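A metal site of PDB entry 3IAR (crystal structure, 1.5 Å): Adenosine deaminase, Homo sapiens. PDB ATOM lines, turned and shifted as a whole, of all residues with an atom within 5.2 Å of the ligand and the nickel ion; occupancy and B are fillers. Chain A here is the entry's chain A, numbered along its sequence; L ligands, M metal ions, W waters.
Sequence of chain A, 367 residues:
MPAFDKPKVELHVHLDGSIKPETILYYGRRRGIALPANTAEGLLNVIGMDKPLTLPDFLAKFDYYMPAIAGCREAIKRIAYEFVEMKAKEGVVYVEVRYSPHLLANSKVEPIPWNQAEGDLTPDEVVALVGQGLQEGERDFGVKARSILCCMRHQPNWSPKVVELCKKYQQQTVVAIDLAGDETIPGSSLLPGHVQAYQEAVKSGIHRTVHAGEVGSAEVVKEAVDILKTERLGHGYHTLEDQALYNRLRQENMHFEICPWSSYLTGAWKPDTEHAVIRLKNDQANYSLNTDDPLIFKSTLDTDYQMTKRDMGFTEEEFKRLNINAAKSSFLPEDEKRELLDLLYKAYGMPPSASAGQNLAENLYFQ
The guanidinium group of Arg 98 lies close to a ring nitrogen (ND1) of His 12 (3.4 Å). NE2 of His 235 lies close to OD2 of Asp 292. OG of Ser 262 sits at hydrogen-bond distance from OD2 of Asp 292 (2.7 Å). The side-chain carboxylate (OE2) of Glu 214 sits at hydrogen-bond distance from a ring nitrogen (NE2) of His 235 (3.2 Å). The backbone NH of Leu 103 is in hydrogen-bond range of the side-chain hydroxyl of Ser 100 (3.2 Å). O of Tyr 99 is in hydrogen-bond range of N of Cys 150 (2.8 Å).
Phe 58 touches the ligand. Leu 59 touches the ligand (CD2 to C3, 3.6 Å). CE1 of Phe 62 touches O3 of the ligand, at 3.6 Å. CA of Tyr 99 touches O1 of the ligand (3.8 Å). Ser 100 touches the ligand. Leu 103 touches the ligand (CD1 to O3, 3.6 Å). Met 152 touches the ligand (CE to C2, 3.7 Å). CB of Ala 180 touches O2 of the ligand, 3.7 Å away. 17 residues have an atom within 4 Å of the ligand: His 12, His 14, Asp 16, Phe 58, Leu 59, Phe 62, Tyr 99, Ser 100, Leu 103, Met 152, Ala 180, Gly 181, His 211, Glu 214, His 235, Asp 292 and Asp 293.
The side-chain carboxylate (OD2) of Asp 16 lies within hydrogen-bond range of an oxygen (O3) of the ligand, at 2.6 Å. OE1 of Glu 214 lies within hydrogen-bond range of N3 of the ligand. The side-chain carboxylate (OD2) of Asp 293 lies within hydrogen-bond range of a nitrogen (N5) of the ligand (2.8 Å). A nitrogen (N4) of the ligand lies close to a ring nitrogen (NE2) of His 235. The backbone NH (N) of Gly 181 is in hydrogen-bond range of a nitrogen (N2) of the ligand (3.1 Å).
Merely in contact with the nickel ion: His 235 (3.8 Å). Of the 23 residues printed, 5 come within 4 Å of the nickel ion. The nearest printed residue that does not touch the nickel ion is Asp 293 (4.3 Å).
The nickel ion is bound by NE2 of His 14, NE2 of His 12, OD1 of Asp 292, N4 of the ligand and NE2 of His 211. The nickel ion has five donor atoms within binding distance.
Water W1 bridges the side-chain carboxylate of Glu 214 (2.8 Å) and the side-chain carboxylate of Asp 292 (2.9 Å).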
ATOM      1  N   HIS A  12      14.892  32.926 -17.641  1.00  0.00           N
ATOM      2  CA  HIS A  12      14.032  32.112 -18.518  1.00  0.00           C
ATOM      3  C   HIS A  12      14.780  31.810 -19.824  1.00  0.00           C
ATOM      4  O   HIS A  12      14.770  32.600 -20.775  1.00  0.00           O
ATOM      5  CB  HIS A  12      12.720  32.851 -18.824  1.00  0.00           C
ATOM      6  CG  HIS A  12      11.739  31.993 -19.550  1.00  0.00           C
ATOM      7  ND1 HIS A  12      10.507  31.663 -19.016  1.00  0.00           N
ATOM      8  CD2 HIS A  12      11.834  31.320 -20.729  1.00  0.00           C
ATOM      9  CE1 HIS A  12       9.861  30.889 -19.861  1.00  0.00           C
ATOM     10  NE2 HIS A  12      10.650  30.629 -20.890  1.00  0.00           N
ATOM     11  N   HIS A  14      16.159  28.138 -22.062  1.00  0.00           N
ATOM     12  CA  HIS A  14      16.097  26.657 -22.099  1.00  0.00           C
ATOM     13  C   HIS A  14      17.454  26.125 -22.611  1.00  0.00           C
ATOM     14  O   HIS A  14      17.954  26.553 -23.661  1.00  0.00           O
ATOM     15  CB  HIS A  14      15.002  26.233 -23.091  1.00  0.00           C
ATOM     16  CG  HIS A  14      13.619  26.647 -22.682  1.00  0.00           C
ATOM     17  ND1 HIS A  14      12.652  25.743 -22.284  1.00  0.00           N
ATOM     18  CD2 HIS A  14      13.009  27.875 -22.640  1.00  0.00           C
ATOM     19  CE1 HIS A  14      11.522  26.383 -22.021  1.00  0.00           C
ATOM     20  NE2 HIS A  14      11.706  27.675 -22.227  1.00  0.00           N
ATOM     21  N   ASP A  16      18.219  23.242 -23.910  1.00  0.00           N
ATOM     22  CA  ASP A  16      18.080  22.565 -25.201  1.00  0.00           C
ATOM     23  C   ASP A  16      17.714  23.532 -26.355  1.00  0.00           C
ATOM     24  O   ASP A  16      17.727  23.166 -27.509  1.00  0.00           O
ATOM     25  CB  ASP A  16      17.110  21.354 -25.125  1.00  0.00           C
ATOM     26  CG  ASP A  16      15.741  21.673 -24.551  1.00  0.00           C
ATOM     27  OD1 ASP A  16      15.492  22.758 -23.984  1.00  0.00           O
ATOM     28  OD2 ASP A  16      14.896  20.734 -24.670  1.00  0.00           O
ATOM     29  N   LEU A  55       3.498  28.685 -31.980  1.00  0.00           N
ATOM     30  CA  LEU A  55       4.250  27.939 -30.959  1.00  0.00           C
ATOM     31  C   LEU A  55       4.521  26.476 -31.410  1.00  0.00           C
ATOM     32  O   LEU A  55       5.632  25.965 -31.272  1.00  0.00           O
ATOM     33  CB  LEU A  55       3.542  28.013 -29.583  1.00  0.00           C
ATOM     34  CG  LEU A  55       4.306  27.387 -28.412  1.00  0.00           C
ATOM     35  CD1 LEU A  55       5.595  28.150 -28.191  1.00  0.00           C
ATOM     36  CD2 LEU A  55       3.472  27.375 -27.112  1.00  0.00           C
ATOM     37  N   PHE A  58       7.370  26.508 -33.909  1.00  0.00           N
ATOM     38  CA  PHE A  58       8.584  26.683 -33.120  1.00  0.00           C
ATOM     39  C   PHE A  58       9.050  25.381 -32.448  1.00  0.00           C
ATOM     40  O   PHE A  58      10.228  24.993 -32.541  1.00  0.00           O
ATOM     41  CB  PHE A  58       8.386  27.818 -32.098  1.00  0.00           C
ATOM     42  CG  PHE A  58       9.296  27.724 -30.922  1.00  0.00           C
ATOM     43  CD1 PHE A  58      10.629  28.030 -31.029  1.00  0.00           C
ATOM     44  CD2 PHE A  58       8.809  27.261 -29.692  1.00  0.00           C
ATOM     45  CE1 PHE A  58      11.467  27.910 -29.965  1.00  0.00           C
ATOM     46  CE2 PHE A  58       9.639  27.151 -28.601  1.00  0.00           C
ATOM     47  CZ  PHE A  58      10.979  27.474 -28.723  1.00  0.00           C
ATOM     48  N   LEU A  59       8.125  24.702 -31.769  1.00  0.00           N
ATOM     49  CA  LEU A  59       8.505  23.498 -31.019  1.00  0.00           C
ATOM     50  C   LEU A  59       9.036  22.413 -31.934  1.00  0.00           C
ATOM     51  O   LEU A  59       9.862  21.600 -31.505  1.00  0.00           O
ATOM     52  CB  LEU A  59       7.304  22.957 -30.230  1.00  0.00           C
ATOM     53  CG  LEU A  59       6.931  23.901 -29.069  1.00  0.00           C
ATOM     54  CD1 LEU A  59       5.569  23.531 -28.468  1.00  0.00           C
ATOM     55  CD2 LEU A  59       8.002  23.812 -27.980  1.00  0.00           C
ATOM     56  N   PHE A  62      13.007  21.650 -32.682  1.00  0.00           N
ATOM     57  CA  PHE A  62      13.835  20.798 -31.840  1.00  0.00           C
ATOM     58  C   PHE A  62      14.106  19.446 -32.495  1.00  0.00           C
ATOM     59  O   PHE A  62      15.166  18.826 -32.233  1.00  0.00           O
ATOM     60  CB  PHE A  62      13.140  20.590 -30.469  1.00  0.00           C
ATOM     61  CG  PHE A  62      13.204  21.799 -29.593  1.00  0.00           C
ATOM     62  CD1 PHE A  62      14.191  21.894 -28.621  1.00  0.00           C
ATOM     63  CD2 PHE A  62      12.303  22.863 -29.770  1.00  0.00           C
ATOM     64  CE1 PHE A  62      14.261  23.034 -27.810  1.00  0.00           C
ATOM     65  CE2 PHE A  62      12.403  23.976 -28.974  1.00  0.00           C
ATOM     66  CZ  PHE A  62      13.380  24.061 -28.005  1.00  0.00           C
ATOM     67  N   MET A  66      17.861  17.751 -31.717  1.00  0.00           N
ATOM     68  CA  MET A  66      17.914  17.041 -30.451  1.00  0.00           C
ATOM     69  C   MET A  66      18.405  15.578 -30.579  1.00  0.00           C
ATOM     70  O   MET A  66      19.090  15.101 -29.673  1.00  0.00           O
ATOM     71  CB  MET A  66      16.565  17.090 -29.734  1.00  0.00           C
ATOM     72  CG  MET A  66      16.192  18.455 -29.158  1.00  0.00           C
ATOM     73  SD  MET A  66      17.277  18.848 -27.749  1.00  0.00           S
ATOM     74  CE  MET A  66      16.385  17.917 -26.470  1.00  0.00           C
ATOM     75  N   ARG A  98      16.827  26.155 -17.829  1.00  0.00           N
ATOM     76  CA  ARG A  98      15.779  25.123 -17.663  1.00  0.00           C
ATOM     77  C   ARG A  98      15.826  24.105 -18.801  1.00  0.00           C
ATOM     78  O   ARG A  98      16.255  24.386 -19.916  1.00  0.00           O
ATOM     79  CB  ARG A  98      14.376  25.776 -17.576  1.00  0.00           C
ATOM     80  CG  ARG A  98      13.882  26.413 -18.846  1.00  0.00           C
ATOM     81  CD  ARG A  98      12.581  27.181 -18.524  1.00  0.00           C
ATOM     82  NE  ARG A  98      12.790  28.263 -17.582  1.00  0.00           N
ATOM     83  CZ  ARG A  98      11.787  28.989 -17.067  1.00  0.00           C
ATOM     84  NH1 ARG A  98      10.524  28.667 -17.396  1.00  0.00           N
ATOM     85  NH2 ARG A  98      12.044  30.009 -16.258  1.00  0.00           N
ATOM     86  N   TYR A  99      15.378  22.888 -18.491  1.00  0.00           N
ATOM     87  CA  TYR A  99      15.321  21.825 -19.502  1.00  0.00           C
ATOM     88  C   TYR A  99      14.494  20.665 -18.971  1.00  0.00           C
ATOM     89  O   TYR A  99      14.240  20.565 -17.747  1.00  0.00           O
ATOM     90  CB  TYR A  99      16.745  21.317 -19.870  1.00  0.00           C
ATOM     91  CG  TYR A  99      17.448  20.655 -18.717  1.00  0.00           C
ATOM     92  CD1 TYR A  99      17.461  19.267 -18.591  1.00  0.00           C
ATOM     93  CD2 TYR A  99      18.034  21.429 -17.698  1.00  0.00           C
ATOM     94  CE1 TYR A  99      18.083  18.648 -17.508  1.00  0.00           C
ATOM     95  CE2 TYR A  99      18.648  20.814 -16.601  1.00  0.00           C
ATOM     96  CZ  TYR A  99      18.638  19.397 -16.507  1.00  0.00           C
ATOM     97  OH  TYR A  99      19.256  18.780 -15.455  1.00  0.00           O
ATOM     98  N   SER A 100      14.045  19.810 -19.880  1.00  0.00           N
ATOM     99  CA  SER A 100      13.414  18.541 -19.524  1.00  0.00           C
ATOM    100  C   SER A 100      14.468  17.442 -19.516  1.00  0.00           C
ATOM    101  O   SER A 100      15.005  17.114 -20.562  1.00  0.00           O
ATOM    102  CB  SER A 100      12.369  18.161 -20.592  1.00  0.00           C
ATOM    103  OG  SER A 100      11.963  16.806 -20.415  1.00  0.00           O
ATOM    104  N   LEU A 103      13.722  14.624 -21.973  1.00  0.00           N
ATOM    105  CA  LEU A 103      13.966  14.837 -23.401  1.00  0.00           C
ATOM    106  C   LEU A 103      15.442  14.644 -23.791  1.00  0.00           C
ATOM    107  O   LEU A 103      15.765  14.661 -24.974  1.00  0.00           O
ATOM    108  CB  LEU A 103      13.451  16.208 -23.860  1.00  0.00           C
ATOM    109  CG  LEU A 103      11.942  16.294 -23.798  1.00  0.00           C
ATOM    110  CD1 LEU A 103      11.569  17.734 -24.214  1.00  0.00           C
ATOM    111  CD2 LEU A 103      11.328  15.299 -24.712  1.00  0.00           C
ATOM    112  N   CYS A 150      11.994  20.998 -16.185  1.00  0.00           N
ATOM    113  CA  CYS A 150      10.664  21.157 -16.788  1.00  0.00           C
ATOM    114  C   CYS A 150       9.807  19.899 -16.803  1.00  0.00           C
ATOM    115  O   CYS A 150      10.200  18.884 -17.404  1.00  0.00           O
ATOM    116  CB  CYS A 150      10.811  21.608 -18.262  1.00  0.00           C
ATOM    117  SG  CYS A 150      11.725  23.150 -18.494  1.00  0.00           S
ATOM    118  N   MET A 152       6.559  18.651 -18.792  1.00  0.00           N
ATOM    119  CA  MET A 152       6.072  18.980 -20.133  1.00  0.00           C
ATOM    120  C   MET A 152       4.562  18.755 -20.208  1.00  0.00           C
ATOM    121  O   MET A 152       4.085  17.724 -19.725  1.00  0.00           O
ATOM    122  CB  MET A 152       6.761  18.078 -21.166  1.00  0.00           C
ATOM    123  CG  MET A 152       8.312  18.316 -21.245  1.00  0.00           C
ATOM    124  SD  MET A 152       8.766  20.035 -21.554  1.00  0.00           S
ATOM    125  CE  MET A 152       8.110  20.201 -23.196  1.00  0.00           C
ATOM    126  N   ALA A 180       6.377  23.407 -19.197  1.00  0.00           N
ATOM    127  CA  ALA A 180       6.609  23.942 -20.514  1.00  0.00           C
ATOM    128  C   ALA A 180       5.865  23.073 -21.541  1.00  0.00           C
ATOM    129  O   ALA A 180       5.139  22.145 -21.165  1.00  0.00           O
ATOM    130  CB  ALA A 180       8.139  24.042 -20.827  1.00  0.00           C
ATOM    131  N   GLY A 181       6.083  23.362 -22.821  1.00  0.00           N
ATOM    132  CA  GLY A 181       5.398  22.630 -23.884  1.00  0.00           C
ATOM    133  C   GLY A 181       4.225  23.423 -24.440  1.00  0.00           C
ATOM    134  O   GLY A 181       4.131  24.658 -24.291  1.00  0.00           O
ATOM    135  N   ASP A 182       3.299  22.698 -25.070  1.00  0.00           N
ATOM    136  CA  ASP A 182       2.213  23.358 -25.795  1.00  0.00           C
ATOM    137  C   ASP A 182       1.073  23.760 -24.864  1.00  0.00           C
ATOM    138  O   ASP A 182       0.260  22.957 -24.399  1.00  0.00           O
ATOM    139  CB  ASP A 182       1.731  22.431 -26.940  1.00  0.00           C
ATOM    140  CG  ASP A 182       0.497  23.007 -27.670  1.00  0.00           C
ATOM    141  OD1 ASP A 182       0.059  24.124 -27.327  1.00  0.00           O
ATOM    142  OD2 ASP A 182      -0.038  22.309 -28.564  1.00  0.00           O
ATOM    143  N   HIS A 211       5.179  28.142 -17.463  1.00  0.00           N
ATOM    144  CA  HIS A 211       4.916  28.855 -18.710  1.00  0.00           C
ATOM    145  C   HIS A 211       3.410  29.054 -18.830  1.00  0.00           C
ATOM    146  O   HIS A 211       2.674  28.060 -18.901  1.00  0.00           O
ATOM    147  CB  HIS A 211       5.361  28.022 -19.899  1.00  0.00           C
ATOM    148  CG  HIS A 211       6.843  28.052 -20.225  1.00  0.00           C
ATOM    149  ND1 HIS A 211       7.820  27.368 -19.495  1.00  0.00           N
ATOM    150  CD2 HIS A 211       7.486  28.580 -21.305  1.00  0.00           C
ATOM    151  CE1 HIS A 211       8.991  27.531 -20.094  1.00  0.00           C
ATOM    152  NE2 HIS A 211       8.816  28.246 -21.197  1.00  0.00           N
ATOM    153  N   GLU A 214       1.578  32.732 -22.639  1.00  0.00           N
ATOM    154  CA  GLU A 214       2.505  32.983 -23.738  1.00  0.00           C
ATOM    155  C   GLU A 214       1.642  33.041 -24.957  1.00  0.00           C
ATOM    156  O   GLU A 214       1.561  34.082 -25.634  1.00  0.00           O
ATOM    157  CB  GLU A 214       3.534  31.864 -23.856  1.00  0.00           C
ATOM    158  CG  GLU A 214       4.504  32.000 -25.066  1.00  0.00           C
ATOM    159  CD  GLU A 214       5.490  30.859 -25.134  1.00  0.00           C
ATOM    160  OE1 GLU A 214       5.391  29.845 -24.343  1.00  0.00           O
ATOM    161  OE2 GLU A 214       6.414  30.915 -25.987  1.00  0.00           O
ATOM    162  N   HIS A 235       6.706  34.075 -19.461  1.00  0.00           N
ATOM    163  CA  HIS A 235       6.005  34.901 -20.442  1.00  0.00           C
ATOM    164  C   HIS A 235       4.895  35.714 -19.775  1.00  0.00           C
ATOM    165  O   HIS A 235       5.128  36.857 -19.371  1.00  0.00           O
ATOM    166  CB  HIS A 235       5.492  34.055 -21.646  1.00  0.00           C
ATOM    167  CG  HIS A 235       6.585  33.362 -22.412  1.00  0.00           C
ATOM    168  ND1 HIS A 235       7.451  34.044 -23.246  1.00  0.00           N
ATOM    169  CD2 HIS A 235       6.922  32.064 -22.491  1.00  0.00           C
ATOM    170  CE1 HIS A 235       8.284  33.176 -23.811  1.00  0.00           C
ATOM    171  NE2 HIS A 235       7.993  31.974 -23.363  1.00  0.00           N
ATOM    172  N   SER A 262      11.622  36.391 -28.436  1.00  0.00           N
ATOM    173  CA  SER A 262      10.891  35.138 -28.489  1.00  0.00           C
ATOM    174  C   SER A 262       9.404  35.385 -28.767  1.00  0.00           C
ATOM    175  O   SER A 262       8.794  34.716 -29.604  1.00  0.00           O
ATOM    176  CB  SER A 262      11.036  34.429 -27.125  1.00  0.00           C
ATOM    177  OG  SER A 262      10.112  33.356 -27.038  1.00  0.00           O
ATOM    178  N   ASP A 292      14.959  32.987 -23.792  1.00  0.00           N
ATOM    179  CA  ASP A 292      14.085  31.813 -23.999  1.00  0.00           C
ATOM    180  C   ASP A 292      14.764  30.693 -24.785  1.00  0.00           C
ATOM    181  O   ASP A 292      15.245  29.702 -24.198  1.00  0.00           O
ATOM    182  CB  ASP A 292      12.728  32.279 -24.629  1.00  0.00           C
ATOM    183  CG  ASP A 292      11.607  31.279 -24.460  1.00  0.00           C
ATOM    184  OD1 ASP A 292      11.714  30.356 -23.604  1.00  0.00           O
ATOM    185  OD2 ASP A 292      10.550  31.490 -25.134  1.00  0.00           O
ATOM    186  N   ASP A 293      14.862  30.839 -26.111  1.00  0.00           N
ATOM    187  CA  ASP A 293      15.479  29.807 -26.949  1.00  0.00           C
ATOM    188  C   ASP A 293      16.393  30.450 -27.994  1.00  0.00           C
ATOM    189  O   ASP A 293      16.112  30.420 -29.191  1.00  0.00           O
ATOM    190  CB  ASP A 293      14.413  28.932 -27.637  1.00  0.00           C
ATOM    191  CG  ASP A 293      13.573  28.171 -26.620  1.00  0.00           C
ATOM    192  OD1 ASP A 293      13.966  27.058 -26.229  1.00  0.00           O
ATOM    193  OD2 ASP A 293      12.565  28.749 -26.115  1.00  0.00           O
HETATM  194  O1  LIG L   1      13.292  23.018 -22.526  1.00  0.00           O
HETATM  195  C1  LIG L   1      12.360  21.923 -22.514  1.00  0.00           C
HETATM  196  C2  LIG L   1      11.365  21.954 -23.672  1.00  0.00           C
HETATM  197  O2  LIG L   1      10.463  23.111 -23.566  1.00  0.00           O
HETATM  198  C3  LIG L   1       9.895  23.421 -24.914  1.00  0.00           C
HETATM  199  N1  LIG L   1       9.987  24.875 -24.893  1.00  0.00           N
HETATM  200  C4  LIG L   1       8.925  25.734 -24.653  1.00  0.00           C
HETATM  201  N2  LIG L   1       7.626  25.413 -24.513  1.00  0.00           N
HETATM  202  C5  LIG L   1       6.868  26.487 -24.342  1.00  0.00           C
HETATM  203  N3  LIG L   1       7.275  27.772 -24.285  1.00  0.00           N
HETATM  204  C6  LIG L   1       8.614  28.067 -24.343  1.00  0.00           C
HETATM  205  N4  LIG L   1       9.026  29.312 -24.095  1.00  0.00           N
HETATM  206  C7  LIG L   1       9.493  26.982 -24.613  1.00  0.00           C
HETATM  207  N5  LIG L   1      10.863  26.936 -24.814  1.00  0.00           N
HETATM  208  C8  LIG L   1      11.128  25.665 -24.980  1.00  0.00           C
HETATM  209  C9  LIG L   1      10.753  22.674 -25.903  1.00  0.00           C
HETATM  210  C10 LIG L   1      11.965  22.146 -25.082  1.00  0.00           C
HETATM  211  O3  LIG L   1      12.437  20.923 -25.608  1.00  0.00           O
HETATM  212 NI    NI M   1      10.377  29.216 -22.420  1.00  0.00          NI
HETATM  213  O   HOH W   1       8.859  29.826 -26.830  1.00  0.00           O
HETATM  214  O   HOH W   2      10.933  19.309 -27.320  1.00  0.00           O
